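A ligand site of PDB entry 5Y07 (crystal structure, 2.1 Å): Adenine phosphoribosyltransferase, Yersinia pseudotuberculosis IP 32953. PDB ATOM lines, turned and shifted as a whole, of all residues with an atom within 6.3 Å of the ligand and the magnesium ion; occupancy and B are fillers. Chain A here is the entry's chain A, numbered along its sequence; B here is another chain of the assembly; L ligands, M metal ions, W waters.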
ATOM      1  N   THR A  67      12.247  24.212 -30.267  1.00  0.00           N
ATOM      2  CA  THR A  67      12.497  23.738 -28.920  1.00  0.00           C
ATOM      3  C   THR A  67      11.390  22.763 -28.521  1.00  0.00           C
ATOM      4  O   THR A  67      10.240  22.997 -28.748  1.00  0.00           O
ATOM      5  CB  THR A  67      12.672  24.906 -27.942  1.00  0.00           C
ATOM      6  OG1 THR A  67      13.743  25.789 -28.397  1.00  0.00           O
ATOM      7  CG2 THR A  67      13.106  24.378 -26.639  1.00  0.00           C
ATOM      8  N   GLU A  68      11.785  21.648 -27.950  1.00  0.00           N
ATOM      9  CA  GLU A  68      10.880  20.636 -27.489  1.00  0.00           C
ATOM     10  C   GLU A  68       9.920  21.179 -26.404  1.00  0.00           C
ATOM     11  O   GLU A  68      10.384  21.973 -25.558  1.00  0.00           O
ATOM     12  CB  GLU A  68      11.684  19.467 -26.912  1.00  0.00           C
ATOM     13  CG  GLU A  68      10.820  18.297 -26.438  1.00  0.00           C
ATOM     14  CD  GLU A  68      11.663  17.119 -25.940  1.00  0.00           C
ATOM     15  OE1 GLU A  68      12.937  17.140 -26.050  1.00  0.00           O
ATOM     16  OE2 GLU A  68      11.040  16.140 -25.560  1.00  0.00           O
ATOM     17  N   ALA A  69       8.638  20.801 -26.429  1.00  0.00           N
ATOM     18  CA  ALA A  69       8.008  20.020 -27.518  1.00  0.00           C
ATOM     19  C   ALA A  69       7.049  20.784 -28.453  1.00  0.00           C
ATOM     20  O   ALA A  69       6.897  20.412 -29.626  1.00  0.00           O
ATOM     21  CB  ALA A  69       7.252  18.842 -26.937  1.00  0.00           C
ATOM     22  N   ARG A  70       6.303  21.783 -27.937  1.00  0.00           N
ATOM     23  CA  ARG A  70       5.306  22.451 -28.793  1.00  0.00           C
ATOM     24  C   ARG A  70       5.974  23.222 -29.913  1.00  0.00           C
ATOM     25  O   ARG A  70       5.388  23.376 -30.954  1.00  0.00           O
ATOM     26  CB  ARG A  70       4.390  23.395 -28.003  1.00  0.00           C
ATOM     27  CG  ARG A  70       3.269  22.668 -27.243  1.00  0.00           C
ATOM     28  CD  ARG A  70       2.269  23.687 -26.592  1.00  0.00           C
ATOM     29  NE  ARG A  70       2.711  24.058 -25.269  1.00  0.00           N
ATOM     30  CZ  ARG A  70       2.626  25.257 -24.692  1.00  0.00           C
ATOM     31  NH1 ARG A  70       2.150  26.330 -25.293  1.00  0.00           N
ATOM     32  NH2 ARG A  70       3.036  25.359 -23.455  1.00  0.00           N
ATOM     33  N   GLY A  71       7.213  23.619 -29.709  1.00  0.00           N
ATOM     34  CA  GLY A  71       7.960  24.354 -30.729  1.00  0.00           C
ATOM     35  C   GLY A  71       8.247  23.440 -31.901  1.00  0.00           C
ATOM     36  O   GLY A  71       8.361  23.917 -33.036  1.00  0.00           O
ATOM     37  N   LYS A  91      14.929  18.395 -24.325  1.00  0.00           N
ATOM     38  CA  LYS A  91      15.097  18.090 -22.926  1.00  0.00           C
ATOM     39  C   LYS A  91      16.199  17.045 -22.774  1.00  0.00           C
ATOM     40  O   LYS A  91      16.530  16.290 -23.717  1.00  0.00           O
ATOM     41  CB  LYS A  91      13.764  17.563 -22.330  1.00  0.00           C
ATOM     42  CG  LYS A  91      12.586  18.563 -22.397  1.00  0.00           C
ATOM     43  CD  LYS A  91      12.878  20.032 -21.995  1.00  0.00           C
ATOM     44  CE  LYS A  91      11.720  21.027 -22.274  1.00  0.00           C
ATOM     45  NZ  LYS A  91      10.428  20.638 -21.559  1.00  0.00           N
ATOM     46  N   TYR A 104      18.156  26.547 -17.537  1.00  0.00           N
ATOM     47  CA  TYR A 104      17.258  27.682 -17.431  1.00  0.00           C
ATOM     48  C   TYR A 104      16.333  27.447 -16.214  1.00  0.00           C
ATOM     49  O   TYR A 104      16.263  26.342 -15.669  1.00  0.00           O
ATOM     50  CB  TYR A 104      16.440  27.936 -18.768  1.00  0.00           C
ATOM     51  CG  TYR A 104      15.409  26.861 -19.187  1.00  0.00           C
ATOM     52  CD1 TYR A 104      15.767  25.513 -19.350  1.00  0.00           C
ATOM     53  CD2 TYR A 104      14.052  27.194 -19.369  1.00  0.00           C
ATOM     54  CE1 TYR A 104      14.840  24.537 -19.678  1.00  0.00           C
ATOM     55  CE2 TYR A 104      13.103  26.199 -19.682  1.00  0.00           C
ATOM     56  CZ  TYR A 104      13.515  24.895 -19.875  1.00  0.00           C
ATOM     57  OH  TYR A 104      12.634  23.977 -20.159  1.00  0.00           O
ATOM     58  N   GLU A 105      15.623  28.526 -15.830  1.00  0.00           N
ATOM     59  CA  GLU A 105      14.735  28.580 -14.647  1.00  0.00           C
ATOM     60  C   GLU A 105      13.295  28.233 -14.971  1.00  0.00           C
ATOM     61  O   GLU A 105      12.646  28.861 -15.840  1.00  0.00           O
ATOM     62  CB  GLU A 105      14.705  30.011 -14.064  1.00  0.00           C
ATOM     63  CG  GLU A 105      16.050  30.624 -13.776  1.00  0.00           C
ATOM     64  CD  GLU A 105      16.660  30.162 -12.444  1.00  0.00           C
ATOM     65  OE1 GLU A 105      16.110  29.199 -11.814  1.00  0.00           O
ATOM     66  OE2 GLU A 105      17.737  30.780 -12.042  1.00  0.00           O
ATOM     67  N   LEU A 106      12.782  27.236 -14.306  1.00  0.00           N
ATOM     68  CA  LEU A 106      11.372  27.003 -14.319  1.00  0.00           C
ATOM     69  C   LEU A 106      10.809  27.738 -13.097  1.00  0.00           C
ATOM     70  O   LEU A 106      11.527  28.381 -12.308  1.00  0.00           O
ATOM     71  CB  LEU A 106      11.069  25.502 -14.351  1.00  0.00           C
ATOM     72  CG  LEU A 106      11.636  24.861 -15.627  1.00  0.00           C
ATOM     73  CD1 LEU A 106      11.652  23.373 -15.483  1.00  0.00           C
ATOM     74  CD2 LEU A 106      10.847  25.287 -16.846  1.00  0.00           C
ATOM     75  N   ASP A 130       9.102  29.024 -31.891  1.00  0.00           N
ATOM     76  CA  ASP A 130       8.412  28.406 -30.735  1.00  0.00           C
ATOM     77  C   ASP A 130       6.950  28.734 -30.868  1.00  0.00           C
ATOM     78  O   ASP A 130       6.539  29.654 -31.661  1.00  0.00           O
ATOM     79  CB  ASP A 130       9.007  28.738 -29.379  1.00  0.00           C
ATOM     80  CG  ASP A 130       8.904  27.553 -28.358  1.00  0.00           C
ATOM     81  OD1 ASP A 130       8.155  26.557 -28.618  1.00  0.00           O
ATOM     82  OD2 ASP A 130       9.554  27.655 -27.274  1.00  0.00           O
ATOM     83  N   ASP A 131       6.102  27.947 -30.200  1.00  0.00           N
ATOM     84  CA  ASP A 131       4.710  28.305 -30.238  1.00  0.00           C
ATOM     85  C   ASP A 131       4.412  29.601 -29.543  1.00  0.00           C
ATOM     86  O   ASP A 131       3.569  30.388 -29.981  1.00  0.00           O
ATOM     87  CB  ASP A 131       3.843  27.197 -29.656  1.00  0.00           C
ATOM     88  CG  ASP A 131       4.108  26.916 -28.173  1.00  0.00           C
ATOM     89  OD1 ASP A 131       5.244  26.890 -27.682  1.00  0.00           O
ATOM     90  OD2 ASP A 131       3.137  26.625 -27.516  1.00  0.00           O
ATOM     91  N   LEU A 132       5.088  29.788 -28.438  1.00  0.00           N
ATOM     92  CA  LEU A 132       4.701  30.791 -27.529  1.00  0.00           C
ATOM     93  C   LEU A 132       5.886  31.463 -26.847  1.00  0.00           C
ATOM     94  O   LEU A 132       6.889  30.795 -26.431  1.00  0.00           O
ATOM     95  CB  LEU A 132       3.659  30.244 -26.514  1.00  0.00           C
ATOM     96  CG  LEU A 132       3.055  31.363 -25.550  1.00  0.00           C
ATOM     97  CD1 LEU A 132       1.544  31.140 -25.448  1.00  0.00           C
ATOM     98  CD2 LEU A 132       3.650  31.267 -24.209  1.00  0.00           C
ATOM     99  N   LEU A 133       5.806  32.812 -26.799  1.00  0.00           N
ATOM    100  CA  LEU A 133       6.764  33.594 -26.110  1.00  0.00           C
ATOM    101  C   LEU A 133       6.122  34.184 -24.845  1.00  0.00           C
ATOM    102  O   LEU A 133       5.086  34.864 -24.962  1.00  0.00           O
ATOM    103  CB  LEU A 133       7.266  34.746 -27.007  1.00  0.00           C
ATOM    104  CG  LEU A 133       8.207  35.709 -26.273  1.00  0.00           C
ATOM    105  CD1 LEU A 133       9.452  34.929 -25.807  1.00  0.00           C
ATOM    106  CD2 LEU A 133       8.542  36.812 -27.254  1.00  0.00           C
ATOM    107  N   ALA A 134       6.679  33.874 -23.661  1.00  0.00           N
ATOM    108  CA  ALA A 134       6.110  34.363 -22.382  1.00  0.00           C
ATOM    109  C   ALA A 134       7.187  35.136 -21.667  1.00  0.00           C
ATOM    110  O   ALA A 134       7.349  36.316 -21.964  1.00  0.00           O
ATOM    111  CB  ALA A 134       5.528  33.200 -21.534  1.00  0.00           C
ATOM    112  N   THR A 135       7.944  34.495 -20.785  1.00  0.00           N
ATOM    113  CA  THR A 135       9.037  35.143 -20.051  1.00  0.00           C
ATOM    114  C   THR A 135      10.311  35.210 -20.837  1.00  0.00           C
ATOM    115  O   THR A 135      11.207  36.025 -20.475  1.00  0.00           O
ATOM    116  CB  THR A 135       9.474  34.438 -18.776  1.00  0.00           C
ATOM    117  OG1 THR A 135      10.192  33.230 -19.141  1.00  0.00           O
ATOM    118  CG2 THR A 135       8.268  34.184 -17.827  1.00  0.00           C
ATOM    119  N   GLY A 136      10.397  34.393 -21.900  1.00  0.00           N
ATOM    120  CA  GLY A 136      11.575  34.301 -22.715  1.00  0.00           C
ATOM    121  C   GLY A 136      12.709  33.405 -22.198  1.00  0.00           C
ATOM    122  O   GLY A 136      13.728  33.321 -22.834  1.00  0.00           O
ATOM    123  N   GLY A 137      12.544  32.671 -21.102  1.00  0.00           N
ATOM    124  CA  GLY A 137      13.651  31.852 -20.494  1.00  0.00           C
ATOM    125  C   GLY A 137      14.068  30.734 -21.470  1.00  0.00           C
ATOM    126  O   GLY A 137      15.209  30.454 -21.685  1.00  0.00           O
ATOM    127  N   THR A 138      13.082  30.131 -22.104  1.00  0.00           N
ATOM    128  CA  THR A 138      13.308  29.008 -23.028  1.00  0.00           C
ATOM    129  C   THR A 138      14.170  29.402 -24.218  1.00  0.00           C
ATOM    130  O   THR A 138      15.221  28.796 -24.518  1.00  0.00           O
ATOM    131  CB  THR A 138      11.887  28.425 -23.425  1.00  0.00           C
ATOM    132  OG1 THR A 138      11.193  27.970 -22.220  1.00  0.00           O
ATOM    133  CG2 THR A 138      12.078  27.284 -24.303  1.00  0.00           C
ATOM    134  N   ILE A 139      13.762  30.460 -24.894  1.00  0.00           N
ATOM    135  CA  ILE A 139      14.502  30.905 -26.063  1.00  0.00           C
ATOM    136  C   ILE A 139      15.844  31.495 -25.676  1.00  0.00           C
ATOM    137  O   ILE A 139      16.785  31.310 -26.392  1.00  0.00           O
ATOM    138  CB  ILE A 139      13.705  31.879 -26.900  1.00  0.00           C
ATOM    139  CG1 ILE A 139      12.427  31.159 -27.418  1.00  0.00           C
ATOM    140  CG2 ILE A 139      14.505  32.427 -28.107  1.00  0.00           C
ATOM    141  CD1 ILE A 139      12.698  29.926 -28.260  1.00  0.00           C
ATOM    142  N   LEU A 165       4.600  39.299 -19.944  1.00  0.00           N
ATOM    143  CA  LEU A 165       5.499  38.439 -19.135  1.00  0.00           C
ATOM    144  C   LEU A 165       6.986  38.792 -19.347  1.00  0.00           C
ATOM    145  O   LEU A 165       7.888  38.207 -18.750  1.00  0.00           O
ATOM    146  CB  LEU A 165       5.139  36.954 -19.394  1.00  0.00           C
ATOM    147  CG  LEU A 165       3.753  36.636 -18.796  1.00  0.00           C
ATOM    148  CD1 LEU A 165       3.217  35.269 -19.170  1.00  0.00           C
ATOM    149  CD2 LEU A 165       3.792  36.775 -17.270  1.00  0.00           C
ATOM    150  N   GLY A 167       9.092  38.499 -22.027  1.00  0.00           N
ATOM    151  CA  GLY A 167       9.992  37.777 -22.917  1.00  0.00           C
ATOM    152  C   GLY A 167      10.409  38.546 -24.171  1.00  0.00           C
ATOM    153  O   GLY A 167      11.579  38.507 -24.555  1.00  0.00           O
ATOM    154  N   GLU B  68       3.945  12.565 -28.545  1.00  0.00           N
ATOM    155  CA  GLU B  68       5.085  13.355 -28.073  1.00  0.00           C
ATOM    156  C   GLU B  68       6.355  12.480 -27.787  1.00  0.00           C
ATOM    157  O   GLU B  68       6.203  11.384 -27.266  1.00  0.00           O
ATOM    158  CB  GLU B  68       4.641  14.096 -26.859  1.00  0.00           C
ATOM    159  CG  GLU B  68       5.753  14.740 -26.041  1.00  0.00           C
ATOM    160  CD  GLU B  68       5.235  15.629 -24.943  1.00  0.00           C
ATOM    161  OE1 GLU B  68       4.010  15.660 -24.539  1.00  0.00           O
ATOM    162  OE2 GLU B  68       6.080  16.385 -24.430  1.00  0.00           O
ATOM    163  N   ARG B  90       0.165  13.380 -25.424  1.00  0.00           N
ATOM    164  CA  ARG B  90       1.222  13.991 -24.719  1.00  0.00           C
ATOM    165  C   ARG B  90       1.574  13.181 -23.439  1.00  0.00           C
ATOM    166  O   ARG B  90       0.755  12.448 -22.926  1.00  0.00           O
ATOM    167  CB  ARG B  90       0.863  15.456 -24.319  1.00  0.00           C
ATOM    168  CG  ARG B  90       0.672  16.389 -25.512  1.00  0.00           C
ATOM    169  CD  ARG B  90       1.131  17.752 -25.300  1.00  0.00           C
ATOM    170  NE  ARG B  90       2.561  17.815 -25.081  1.00  0.00           N
ATOM    171  CZ  ARG B  90       3.192  18.944 -24.762  1.00  0.00           C
ATOM    172  NH1 ARG B  90       2.541  20.145 -24.722  1.00  0.00           N
ATOM    173  NH2 ARG B  90       4.477  18.904 -24.500  1.00  0.00           N
ATOM    174  N   LYS B  94       0.531  18.189 -19.515  1.00  0.00           N
ATOM    175  CA  LYS B  94       0.930  19.221 -20.528  1.00  0.00           C
ATOM    176  C   LYS B  94      -0.323  19.702 -21.272  1.00  0.00           C
ATOM    177  O   LYS B  94      -0.298  20.785 -21.821  1.00  0.00           O
ATOM    178  CB  LYS B  94       1.956  18.645 -21.481  1.00  0.00           C
ATOM    179  CG  LYS B  94       3.348  18.321 -20.886  1.00  0.00           C
ATOM    180  CD  LYS B  94       3.979  19.525 -20.171  1.00  0.00           C
ATOM    181  CE  LYS B  94       4.272  20.727 -21.092  1.00  0.00           C
ATOM    182  NZ  LYS B  94       4.780  21.948 -20.372  1.00  0.00           N
HETATM  183  C1  LIG L   1       6.166  26.590 -23.213  1.00  0.00           C
HETATM  184  C2  LIG L   1       6.051  27.057 -24.701  1.00  0.00           C
HETATM  185  C3  LIG L   1       7.443  27.698 -24.889  1.00  0.00           C
HETATM  186  C4  LIG L   1       7.784  28.282 -23.499  1.00  0.00           C
HETATM  187  C5  LIG L   1       7.495  29.775 -23.335  1.00  0.00           C
HETATM  188  O1  LIG L   1       6.895  25.371 -23.200  1.00  0.00           O
HETATM  189  O2  LIG L   1       5.920  25.905 -25.524  1.00  0.00           O
HETATM  190  O3  LIG L   1       8.532  26.731 -25.193  1.00  0.00           O
HETATM  191  O4  LIG L   1       6.973  27.545 -22.564  1.00  0.00           O
HETATM  192  O5  LIG L   1       7.719  30.214 -21.940  1.00  0.00           O
HETATM  193  P1  LIG L   1       8.973  31.185 -21.532  1.00  0.00           P
HETATM  194  O6  LIG L   1       8.424  31.667 -20.192  1.00  0.00           O
HETATM  195  O7  LIG L   1      10.236  30.308 -21.418  1.00  0.00           O
HETATM  196  O8  LIG L   1       8.947  32.092 -22.756  1.00  0.00           O
HETATM  197  P2  LIG L   1       6.738  24.166 -22.053  1.00  0.00           P
HETATM  198  O9  LIG L   1       8.141  23.842 -21.467  1.00  0.00           O
HETATM  199  O10 LIG L   1       5.662  24.475 -20.960  1.00  0.00           O
HETATM  200  O11 LIG L   1       6.181  22.746 -22.624  1.00  0.00           O
HETATM  201  P3  LIG L   1       6.141  22.015 -24.056  1.00  0.00           P
HETATM  202  O12 LIG L   1       4.679  21.761 -24.186  1.00  0.00           O
HETATM  203  O13 LIG L   1       6.760  22.887 -25.194  1.00  0.00           O
HETATM  204  O14 LIG L   1       6.803  20.665 -23.770  1.00  0.00           O
HETATM  205 MG    MG M   1       7.712  24.675 -25.046  1.00  0.00          MG
HETATM  206  O   HOH W   1      11.043  31.678 -24.509  1.00  0.00           O
HETATM  207  O   HOH W   2       9.379  24.020 -24.123  1.00  0.00           O
HETATM  208  O   HOH W   3      10.567  25.194 -22.133  1.00  0.00           O
HETATM  209  O   HOH W   4      10.667  29.455 -19.041  1.00  0.00           O
HETATM  210  O   HOH W   5       8.297  24.508 -27.136  1.00  0.00           O
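O7 of the ligand is in hydrogen-bond range of N of Gly 137 (3.3 Å).
N of Ala 69 sits at hydrogen-bond distance from O14 of the ligand (3.2 Å).
The side-chain amino group (NZ) of Lys 91 lies within salt-bridge range of an oxygen (O9) of the ligand.
The side-chain amino group of Lys 94 of chain B is in salt-bridge range of an oxygen (O10) of the ligand (2.7 Å).
OD2 of Asp 130 lies close to O3 of the ligand (2.5 Å).
An oxygen (O6) of the ligand lies within hydrogen-bond range of the backbone NH (N) of Thr 135 (2.9 Å).
O7 of the ligand is in hydrogen-bond range of N of Thr 138 (2.9 Å).
The guanidinium group of Arg 70 lies within salt-bridge range of an oxygen (O12) of the ligand.
The guanidinium group (NH1) of Arg 90 of chain B lies within salt-bridge range of an oxygen (O12) of the ligand (2.7 Å).
OG1 of Thr 135 sits at hydrogen-bond distance from O6 of the ligand (2.6 Å).
An oxygen (O7) of the ligand lies within hydrogen-bond range of the side-chain hydroxyl of Thr 138 (2.7 Å).
The backbone NH of Gly 136 lies within hydrogen-bond range of an oxygen (O8) of the ligand (2.9 Å).
The backbone NH (N) of Ala 134 lies within hydrogen-bond range of an oxygen (O8) of the ligand (3.0 Å).
OD1 of Asp 131 lies close to O2 of the ligand.
The backbone NH (N) of Arg 70 lies close to an oxygen (O13) of the ligand (3.0 Å).
The backbone NH (N) of Gly 71 sits close to the side-chain carboxylate (OD1) of Asp 130, 3.3 Å away.
The guanidinium group of Arg 90 of chain B is in salt-bridge range of the side-chain carboxylate of Glu 68 of chain B, 2.7 Å away.
N of Lys 91 sits at hydrogen-bond distance from OE1 of Glu 68 of chain A (2.9 Å).
O of Ala 134 is in hydrogen-bond range of N of Gly 167, at 2.8 Å.
The side-chain hydroxyl (OG1) of Thr 135 sits at hydrogen-bond distance from the backbone NH (N) of Gly 137 (3.1 Å).
OD2 of Asp 131 is in salt-bridge range of NH1 of Arg 70 (2.5 Å).
Merely in contact with the ligand: Glu 68 of chain A (3.8 Å) and Leu 132 (3.3 Å).
Along chain A the residues within 4 Å of the ligand span positions 68 to 138.
Glu 68 of chain A touches the magnesium ion.
Of the 24 residues printed, 1 comes within 4 Å of the magnesium ion.
The nearest printed residue that does not touch the magnesium ion is Asp 130 (4.1 Å).
The magnesium ion is bound by water W2 (2.0 Å).
The magnesium ion is bound by an oxygen (O13) of the ligand, at 2.0 Å.
O1 of the ligand binds the magnesium ion (2.1 Å).
Water W5 is bound to the magnesium ion (2.2 Å).
O3 of the ligand binds the magnesium ion, 2.2 Å away.
O2 of the ligand binds the magnesium ion (2.2 Å).
Water W5 lies within hydrogen-bond range of OD1 of Asp 130 (2.5 Å), N of Gly 71 (2.9 Å), O of Thr 67 (2.9 Å) and N of Arg 70 (3.5 Å).
Water W2 lies within hydrogen-bond range of the backbone carbonyl oxygen (O) of Glu 68 of chain A and an oxygen (O9) of the ligand.
Water W1 lies within hydrogen-bond range of an oxygen (O8) of the ligand (2.8 Å) and the backbone NH (N) of Ile 139 (3.0 Å).
Water W3 lies within hydrogen-bond range of the side-chain hydroxyl of Thr 138 (2.8 Å), an oxygen (O9) of the ligand (2.9 Å) and the side-chain hydroxyl of Tyr 104 (3.1 Å).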
